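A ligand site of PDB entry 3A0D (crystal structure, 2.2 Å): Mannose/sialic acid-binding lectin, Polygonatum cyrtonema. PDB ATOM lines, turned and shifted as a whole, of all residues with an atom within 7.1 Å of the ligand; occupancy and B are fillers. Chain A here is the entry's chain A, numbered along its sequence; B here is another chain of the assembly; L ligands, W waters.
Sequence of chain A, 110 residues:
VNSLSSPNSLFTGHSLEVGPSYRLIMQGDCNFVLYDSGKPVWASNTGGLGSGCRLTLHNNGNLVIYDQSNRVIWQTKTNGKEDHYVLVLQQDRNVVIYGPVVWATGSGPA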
ATOM      1  N   GLN A  90      27.492  20.034  14.561  1.00  0.00           N
ATOM      2  CA  GLN A  90      26.540  19.792  15.636  1.00  0.00           C
ATOM      3  C   GLN A  90      25.592  18.618  15.437  1.00  0.00           C
ATOM      4  O   GLN A  90      25.359  18.156  14.311  1.00  0.00           O
ATOM      5  CB  GLN A  90      25.733  21.075  15.875  1.00  0.00           C
ATOM      6  CG  GLN A  90      26.624  22.262  16.230  1.00  0.00           C
ATOM      7  CD  GLN A  90      25.836  23.527  16.536  1.00  0.00           C
ATOM      8  OE1 GLN A  90      26.353  24.435  17.182  1.00  0.00           O
ATOM      9  NE2 GLN A  90      24.599  23.604  16.051  1.00  0.00           N
ATOM     10  N   ASP A  92      22.602  18.745  15.622  1.00  0.00           N
ATOM     11  CA  ASP A  92      21.423  19.221  14.906  1.00  0.00           C
ATOM     12  C   ASP A  92      21.771  19.324  13.423  1.00  0.00           C
ATOM     13  O   ASP A  92      20.985  19.811  12.610  1.00  0.00           O
ATOM     14  CB  ASP A  92      20.921  20.561  15.473  1.00  0.00           C
ATOM     15  CG  ASP A  92      21.817  21.740  15.110  1.00  0.00           C
ATOM     16  OD1 ASP A  92      22.975  21.539  14.687  1.00  0.00           O
ATOM     17  OD2 ASP A  92      21.358  22.897  15.275  1.00  0.00           O
ATOM     18  N   ARG A  93      22.973  18.848  13.094  1.00  0.00           N
ATOM     19  CA  ARG A  93      23.521  18.812  11.730  1.00  0.00           C
ATOM     20  C   ARG A  93      24.020  20.129  11.149  1.00  0.00           C
ATOM     21  O   ARG A  93      24.448  20.179   9.986  1.00  0.00           O
ATOM     22  CB  ARG A  93      22.508  18.189  10.753  1.00  0.00           C
ATOM     23  CG  ARG A  93      23.167  17.524   9.559  1.00  0.00           C
ATOM     24  CD  ARG A  93      22.159  16.967   8.551  1.00  0.00           C
ATOM     25  NE  ARG A  93      21.519  18.028   7.785  1.00  0.00           N
ATOM     26  CZ  ARG A  93      20.685  17.800   6.765  1.00  0.00           C
ATOM     27  NH1 ARG A  93      20.397  16.569   6.393  1.00  0.00           N
ATOM     28  NH2 ARG A  93      20.157  18.828   6.107  1.00  0.00           N
ATOM     29  N   ASN A  94      23.966  21.195  11.931  1.00  0.00           N
ATOM     30  CA  ASN A  94      24.450  22.484  11.455  1.00  0.00           C
ATOM     31  C   ASN A  94      25.969  22.485  11.693  1.00  0.00           C
ATOM     32  O   ASN A  94      26.445  21.800  12.606  1.00  0.00           O
ATOM     33  CB  ASN A  94      23.794  23.618  12.233  1.00  0.00           C
ATOM     34  CG  ASN A  94      23.798  24.938  11.466  1.00  0.00           C
ATOM     35  OD1 ASN A  94      24.302  25.011  10.352  1.00  0.00           O
ATOM     36  ND2 ASN A  94      23.230  25.978  12.058  1.00  0.00           N
ATOM     37  N   VAL A  95      26.713  23.204  10.857  1.00  0.00           N
ATOM     38  CA  VAL A  95      28.166  23.314  10.987  1.00  0.00           C
ATOM     39  C   VAL A  95      28.383  24.784  11.292  1.00  0.00           C
ATOM     40  O   VAL A  95      28.034  25.653  10.493  1.00  0.00           O
ATOM     41  CB  VAL A  95      28.885  22.911   9.680  1.00  0.00           C
ATOM     42  CG1 VAL A  95      30.388  23.187   9.799  1.00  0.00           C
ATOM     43  CG2 VAL A  95      28.664  21.425   9.401  1.00  0.00           C
ATOM     44  N   VAL A  96      28.970  25.062  12.455  1.00  0.00           N
ATOM     45  CA  VAL A  96      29.125  26.439  12.889  1.00  0.00           C
ATOM     46  C   VAL A  96      30.484  26.866  13.423  1.00  0.00           C
ATOM     47  O   VAL A  96      31.183  26.090  14.079  1.00  0.00           O
ATOM     48  CB  VAL A  96      28.083  26.732  13.998  1.00  0.00           C
ATOM     49  CG1 VAL A  96      28.032  28.227  14.306  1.00  0.00           C
ATOM     50  CG2 VAL A  96      26.725  26.191  13.585  1.00  0.00           C
ATOM     51  N   ILE A  97      30.838  28.119  13.150  1.00  0.00           N
ATOM     52  CA  ILE A  97      32.071  28.696  13.656  1.00  0.00           C
ATOM     53  C   ILE A  97      31.654  29.612  14.805  1.00  0.00           C
ATOM     54  O   ILE A  97      30.816  30.499  14.619  1.00  0.00           O
ATOM     55  CB  ILE A  97      32.798  29.563  12.605  1.00  0.00           C
ATOM     56  CG1 ILE A  97      33.281  28.689  11.442  1.00  0.00           C
ATOM     57  CG2 ILE A  97      33.985  30.279  13.243  1.00  0.00           C
ATOM     58  CD1 ILE A  97      33.991  29.470  10.344  1.00  0.00           C
ATOM     59  N   TYR A  98      32.217  29.382  15.986  1.00  0.00           N
ATOM     60  CA  TYR A  98      31.902  30.200  17.161  1.00  0.00           C
ATOM     61  C   TYR A  98      33.152  30.886  17.675  1.00  0.00           C
ATOM     62  O   TYR A  98      34.255  30.344  17.556  1.00  0.00           O
ATOM     63  CB  TYR A  98      31.348  29.373  18.313  1.00  0.00           C
ATOM     64  CG  TYR A  98      30.001  28.735  18.081  1.00  0.00           C
ATOM     65  CD1 TYR A  98      29.885  27.445  17.556  1.00  0.00           C
ATOM     66  CD2 TYR A  98      28.826  29.398  18.456  1.00  0.00           C
ATOM     67  CE1 TYR A  98      28.650  26.825  17.430  1.00  0.00           C
ATOM     68  CE2 TYR A  98      27.588  28.786  18.334  1.00  0.00           C
ATOM     69  CZ  TYR A  98      27.502  27.502  17.817  1.00  0.00           C
ATOM     70  OH  TYR A  98      26.285  26.882  17.701  1.00  0.00           O
ATOM     71  N   SER B   5      26.076  22.576  22.476  1.00  0.00           N
ATOM     72  CA  SER B   5      25.660  23.854  21.932  1.00  0.00           C
ATOM     73  C   SER B   5      24.446  24.421  22.652  1.00  0.00           C
ATOM     74  O   SER B   5      23.511  23.684  22.967  1.00  0.00           O
ATOM     75  CB  SER B   5      25.356  23.712  20.441  1.00  0.00           C
ATOM     76  OG  SER B   5      26.504  23.297  19.729  1.00  0.00           O
ATOM     77  N   SER B   6      24.465  25.718  22.907  1.00  0.00           N
ATOM     78  CA  SER B   6      23.343  26.374  23.568  1.00  0.00           C
ATOM     79  C   SER B   6      22.138  26.180  22.665  1.00  0.00           C
ATOM     80  O   SER B   6      22.273  26.119  21.432  1.00  0.00           O
ATOM     81  CB  SER B   6      23.623  27.864  23.746  1.00  0.00           C
ATOM     82  OG  SER B   6      23.709  28.527  22.491  1.00  0.00           O
ATOM     83  N   PRO B   7      20.932  26.103  23.237  1.00  0.00           N
ATOM     84  CA  PRO B   7      20.618  26.191  24.676  1.00  0.00           C
ATOM     85  C   PRO B   7      20.482  24.814  25.312  1.00  0.00           C
ATOM     86  O   PRO B   7      19.844  24.669  26.364  1.00  0.00           O
ATOM     87  CB  PRO B   7      19.304  26.931  24.672  1.00  0.00           C
ATOM     88  CG  PRO B   7      18.603  26.272  23.502  1.00  0.00           C
ATOM     89  CD  PRO B   7      19.697  26.177  22.435  1.00  0.00           C
ATOM     90  N   ASN B   8      21.099  23.816  24.696  1.00  0.00           N
ATOM     91  CA  ASN B   8      21.009  22.434  25.176  1.00  0.00           C
ATOM     92  C   ASN B   8      21.692  22.111  26.492  1.00  0.00           C
ATOM     93  O   ASN B   8      22.504  22.878  26.996  1.00  0.00           O
ATOM     94  CB  ASN B   8      21.502  21.492  24.077  1.00  0.00           C
ATOM     95  CG  ASN B   8      20.804  21.746  22.769  1.00  0.00           C
ATOM     96  OD1 ASN B   8      19.575  21.834  22.723  1.00  0.00           O
ATOM     97  ND2 ASN B   8      21.575  21.881  21.689  1.00  0.00           N
ATOM     98  N   ASN B  59      21.864  30.593  25.570  1.00  0.00           N
ATOM     99  CA  ASN B  59      22.075  31.335  24.336  1.00  0.00           C
ATOM    100  C   ASN B  59      22.734  32.688  24.546  1.00  0.00           C
ATOM    101  O   ASN B  59      22.930  33.449  23.593  1.00  0.00           O
ATOM    102  CB  ASN B  59      20.747  31.514  23.588  1.00  0.00           C
ATOM    103  CG  ASN B  59      20.261  30.221  22.944  1.00  0.00           C
ATOM    104  OD1 ASN B  59      21.061  29.384  22.541  1.00  0.00           O
ATOM    105  ND2 ASN B  59      18.944  30.071  22.821  1.00  0.00           N
ATOM    106  N   ASP B  83      22.452  35.177  21.481  1.00  0.00           N
ATOM    107  CA  ASP B  83      22.771  34.590  20.192  1.00  0.00           C
ATOM    108  C   ASP B  83      22.821  33.071  20.360  1.00  0.00           C
ATOM    109  O   ASP B  83      21.830  32.440  20.708  1.00  0.00           O
ATOM    110  CB  ASP B  83      24.125  35.125  19.705  1.00  0.00           C
ATOM    111  CG  ASP B  83      24.330  34.930  18.219  1.00  0.00           C
ATOM    112  OD1 ASP B  83      25.319  34.273  17.825  1.00  0.00           O
ATOM    113  OD2 ASP B  83      23.510  35.456  17.443  1.00  0.00           O
ATOM    114  N   HIS B  84      23.992  32.482  20.108  1.00  0.00           N
ATOM    115  CA  HIS B  84      24.213  31.056  20.278  1.00  0.00           C
ATOM    116  C   HIS B  84      25.672  30.806  20.609  1.00  0.00           C
ATOM    117  O   HIS B  84      26.560  31.477  20.080  1.00  0.00           O
ATOM    118  CB  HIS B  84      23.818  30.274  19.025  1.00  0.00           C
ATOM    119  CG  HIS B  84      22.346  30.075  18.873  1.00  0.00           C
ATOM    120  ND1 HIS B  84      21.537  30.938  18.164  1.00  0.00           N
ATOM    121  CD2 HIS B  84      21.512  29.138  19.398  1.00  0.00           C
ATOM    122  CE1 HIS B  84      20.282  30.557  18.260  1.00  0.00           C
ATOM    123  NE2 HIS B  84      20.229  29.461  19.002  1.00  0.00           N
ATOM    124  N   TYR B  85      25.924  29.855  21.497  1.00  0.00           N
ATOM    125  CA  TYR B  85      27.279  29.536  21.909  1.00  0.00           C
ATOM    126  C   TYR B  85      27.511  28.033  21.945  1.00  0.00           C
ATOM    127  O   TYR B  85      26.587  27.248  21.749  1.00  0.00           O
ATOM    128  CB  TYR B  85      27.549  30.125  23.302  1.00  0.00           C
ATOM    129  CG  TYR B  85      27.426  31.629  23.356  1.00  0.00           C
ATOM    130  CD1 TYR B  85      26.181  32.255  23.279  1.00  0.00           C
ATOM    131  CD2 TYR B  85      28.558  32.444  23.433  1.00  0.00           C
ATOM    132  CE1 TYR B  85      26.056  33.641  23.284  1.00  0.00           C
ATOM    133  CE2 TYR B  85      28.457  33.827  23.436  1.00  0.00           C
ATOM    134  CZ  TYR B  85      27.204  34.417  23.354  1.00  0.00           C
ATOM    135  OH  TYR B  85      27.108  35.794  23.329  1.00  0.00           O
ATOM    136  N   VAL B 101      27.956  33.433  17.260  1.00  0.00           N
ATOM    137  CA  VAL B 101      28.085  32.822  15.940  1.00  0.00           C
ATOM    138  C   VAL B 101      28.833  33.724  14.969  1.00  0.00           C
ATOM    139  O   VAL B 101      28.528  34.911  14.833  1.00  0.00           O
ATOM    140  CB  VAL B 101      26.709  32.490  15.331  1.00  0.00           C
ATOM    141  CG1 VAL B 101      26.873  31.972  13.908  1.00  0.00           C
ATOM    142  CG2 VAL B 101      25.988  31.461  16.181  1.00  0.00           C
ATOM    143  N   VAL B 102      29.823  33.151  14.294  1.00  0.00           N
ATOM    144  CA  VAL B 102      30.618  33.873  13.311  1.00  0.00           C
ATOM    145  C   VAL B 102      30.177  33.506  11.904  1.00  0.00           C
ATOM    146  O   VAL B 102      30.136  34.352  11.016  1.00  0.00           O
ATOM    147  CB  VAL B 102      32.125  33.534  13.465  1.00  0.00           C
ATOM    148  CG1 VAL B 102      32.896  33.976  12.217  1.00  0.00           C
ATOM    149  CG2 VAL B 102      32.690  34.227  14.707  1.00  0.00           C
ATOM    150  N   TRP B 103      29.845  32.234  11.708  1.00  0.00           N
ATOM    151  CA  TRP B 103      29.438  31.725  10.407  1.00  0.00           C
ATOM    152  C   TRP B 103      28.742  30.378  10.593  1.00  0.00           C
ATOM    153  O   TRP B 103      29.017  29.670  11.553  1.00  0.00           O
ATOM    154  CB  TRP B 103      30.698  31.534   9.554  1.00  0.00           C
ATOM    155  CG  TRP B 103      30.471  30.945   8.186  1.00  0.00           C
ATOM    156  CD1 TRP B 103      30.139  31.625   7.049  1.00  0.00           C
ATOM    157  CD2 TRP B 103      30.605  29.574   7.812  1.00  0.00           C
ATOM    158  NE1 TRP B 103      30.065  30.755   5.983  1.00  0.00           N
ATOM    159  CE2 TRP B 103      30.347  29.490   6.419  1.00  0.00           C
ATOM    160  CE3 TRP B 103      30.928  28.407   8.509  1.00  0.00           C
ATOM    161  CZ2 TRP B 103      30.400  28.282   5.722  1.00  0.00           C
ATOM    162  CZ3 TRP B 103      30.973  27.198   7.807  1.00  0.00           C
ATOM    163  CH2 TRP B 103      30.712  27.147   6.438  1.00  0.00           C
ATOM    164  N   ALA B 104      27.857  30.035   9.665  1.00  0.00           N
ATOM    165  CA  ALA B 104      27.139  28.761   9.728  1.00  0.00           C
ATOM    166  C   ALA B 104      26.787  28.298   8.313  1.00  0.00           C
ATOM    167  O   ALA B 104      26.533  29.113   7.433  1.00  0.00           O
ATOM    168  CB  ALA B 104      25.881  28.904  10.560  1.00  0.00           C
ATOM    169  N   THR B 105      26.774  26.987   8.107  1.00  0.00           N
ATOM    170  CA  THR B 105      26.440  26.421   6.803  1.00  0.00           C
ATOM    171  C   THR B 105      24.940  26.473   6.589  1.00  0.00           C
ATOM    172  O   THR B 105      24.463  26.546   5.464  1.00  0.00           O
ATOM    173  CB  THR B 105      26.858  24.953   6.698  1.00  0.00           C
ATOM    174  OG1 THR B 105      26.214  24.214   7.741  1.00  0.00           O
ATOM    175  CG2 THR B 105      28.367  24.810   6.822  1.00  0.00           C
ATOM    176  N   GLY B 106      24.192  26.396   7.685  1.00  0.00           N
ATOM    177  CA  GLY B 106      22.750  26.402   7.593  1.00  0.00           C
ATOM    178  C   GLY B 106      22.242  25.022   7.244  1.00  0.00           C
ATOM    179  O   GLY B 106      21.097  24.866   6.829  1.00  0.00           O
ATOM    180  N   GLY B 108      21.604  22.817   9.239  1.00  0.00           N
ATOM    181  CA  GLY B 108      20.821  22.375  10.370  1.00  0.00           C
ATOM    182  C   GLY B 108      20.185  23.603  11.010  1.00  0.00           C
ATOM    183  O   GLY B 108      20.543  24.721  10.637  1.00  0.00           O
ATOM    184  N   PRO B 109      19.263  23.445  11.972  1.00  0.00           N
ATOM    185  CA  PRO B 109      18.768  22.168  12.505  1.00  0.00           C
ATOM    186  C   PRO B 109      17.983  21.350  11.483  1.00  0.00           C
ATOM    187  O   PRO B 109      17.140  21.871  10.746  1.00  0.00           O
ATOM    188  CB  PRO B 109      17.912  22.603  13.688  1.00  0.00           C
ATOM    189  CG  PRO B 109      17.408  23.935  13.272  1.00  0.00           C
ATOM    190  CD  PRO B 109      18.637  24.570  12.678  1.00  0.00           C
HETATM  191  C1  LIG L   1      20.782  27.412  14.648  1.00  0.00           C
HETATM  192  C2  LIG L   1      21.427  26.344  15.563  1.00  0.00           C
HETATM  193  C3  LIG L   1      22.459  27.027  16.486  1.00  0.00           C
HETATM  194  C4  LIG L   1      23.522  27.693  15.601  1.00  0.00           C
HETATM  195  C5  LIG L   1      22.838  28.719  14.674  1.00  0.00           C
HETATM  196  C6  LIG L   1      23.899  29.368  13.774  1.00  0.00           C
HETATM  197  C7  LIG L   1      19.463  29.364  14.588  1.00  0.00           C
HETATM  198  O1  LIG L   1      20.079  28.397  15.451  1.00  0.00           O
HETATM  199  O2  LIG L   1      22.106  25.362  14.761  1.00  0.00           O
HETATM  200  O3  LIG L   1      23.072  26.056  17.333  1.00  0.00           O
HETATM  201  O4  LIG L   1      24.483  28.357  16.428  1.00  0.00           O
HETATM  202  O5  LIG L   1      21.845  28.058  13.843  1.00  0.00           O
HETATM  203  O6  LIG L   1      23.277  30.313  12.903  1.00  0.00           O
HETATM  204  O   HOH W   1      21.007  25.099  19.242  1.00  0.00           O
HETATM  205  O   HOH W   2      17.541  28.068  11.966  1.00  0.00           O
HETATM  206  O   HOH W   3      22.665  32.720  13.932  1.00  0.00           O
HETATM  207  O   HOH W   4      18.332  26.746  17.022  1.00  0.00           O
HETATM  208  O   HOH W   5      22.370  28.621  10.621  1.00  0.00           O
HETATM  209  O   HOH W   6      24.217  26.914  19.676  1.00  0.00           O
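OD1 of Asp 92 is in hydrogen-bond range of N of Asn 94 (2.9 Å). OD1 of Asp 92 is in hydrogen-bond range of NE2 of Gln 90, 3.0 Å away. The side-chain amide oxygen (OE1) of Gln 90 is in hydrogen-bond range of the side-chain hydroxyl (OH) of Tyr 98 (2.5 Å). ND2 of Asn 94 is in hydrogen-bond range of O of Gly 108 of chain B, at 3.3 Å. The backbone NH (N) of Gly 106 of chain B lies within hydrogen-bond range of the side-chain amide oxygen (OD1) of Asn 94, 3.0 Å away. OD1 of Asn 94 lies within hydrogen-bond range of OG1 of Thr 105 of chain B (3.3 Å). OG of Ser 5 of chain B is in hydrogen-bond range of OE1 of Gln 90, at 2.8 Å. N of Val 101 of chain B lies within hydrogen-bond range of OD1 of Asp 83 of chain B (2.8 Å).
CB of His 84 of chain B touches O4 of the ligand, at 3.3 Å. Val 101 of chain B touches the ligand (CG2 to O4, 3.5 Å). Ala 104 of chain B touches the ligand. Of the 24 residues printed, 7 come within 4 Å of the ligand. The nearest printed residue that does not touch the ligand is Pro 109 of chain B (4.1 Å).
Water W6 lies within hydrogen-bond range of the backbone carbonyl oxygen (O) of Ser 6 of chain B (2.7 Å), an oxygen (O3) of the ligand (2.7 Å), the side-chain hydroxyl (OH) of Tyr 98 (2.9 Å) and the backbone carbonyl oxygen (O) of Tyr 85 of chain B (3.2 Å). Water W1 bridges O of Ser 6 of chain B and O3 of the ligand. Water W5 bridges O6 of the ligand and ND2 of Asn 94.
The side-chain carboxylate of Asp 92 lies within hydrogen-bond range of an oxygen (O2) of the ligand (2.6 Å). The side-chain hydroxyl (OH) of Tyr 98 sits at hydrogen-bond distance from an oxygen (O4) of the ligand. The side-chain amide nitrogen (ND2) of Asn 94 lies within hydrogen-bond range of an oxygen (O2) of the ligand. The side-chain amide nitrogen of Gln 90 sits at hydrogen-bond distance from an oxygen (O3) of the ligand (3.2 Å).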
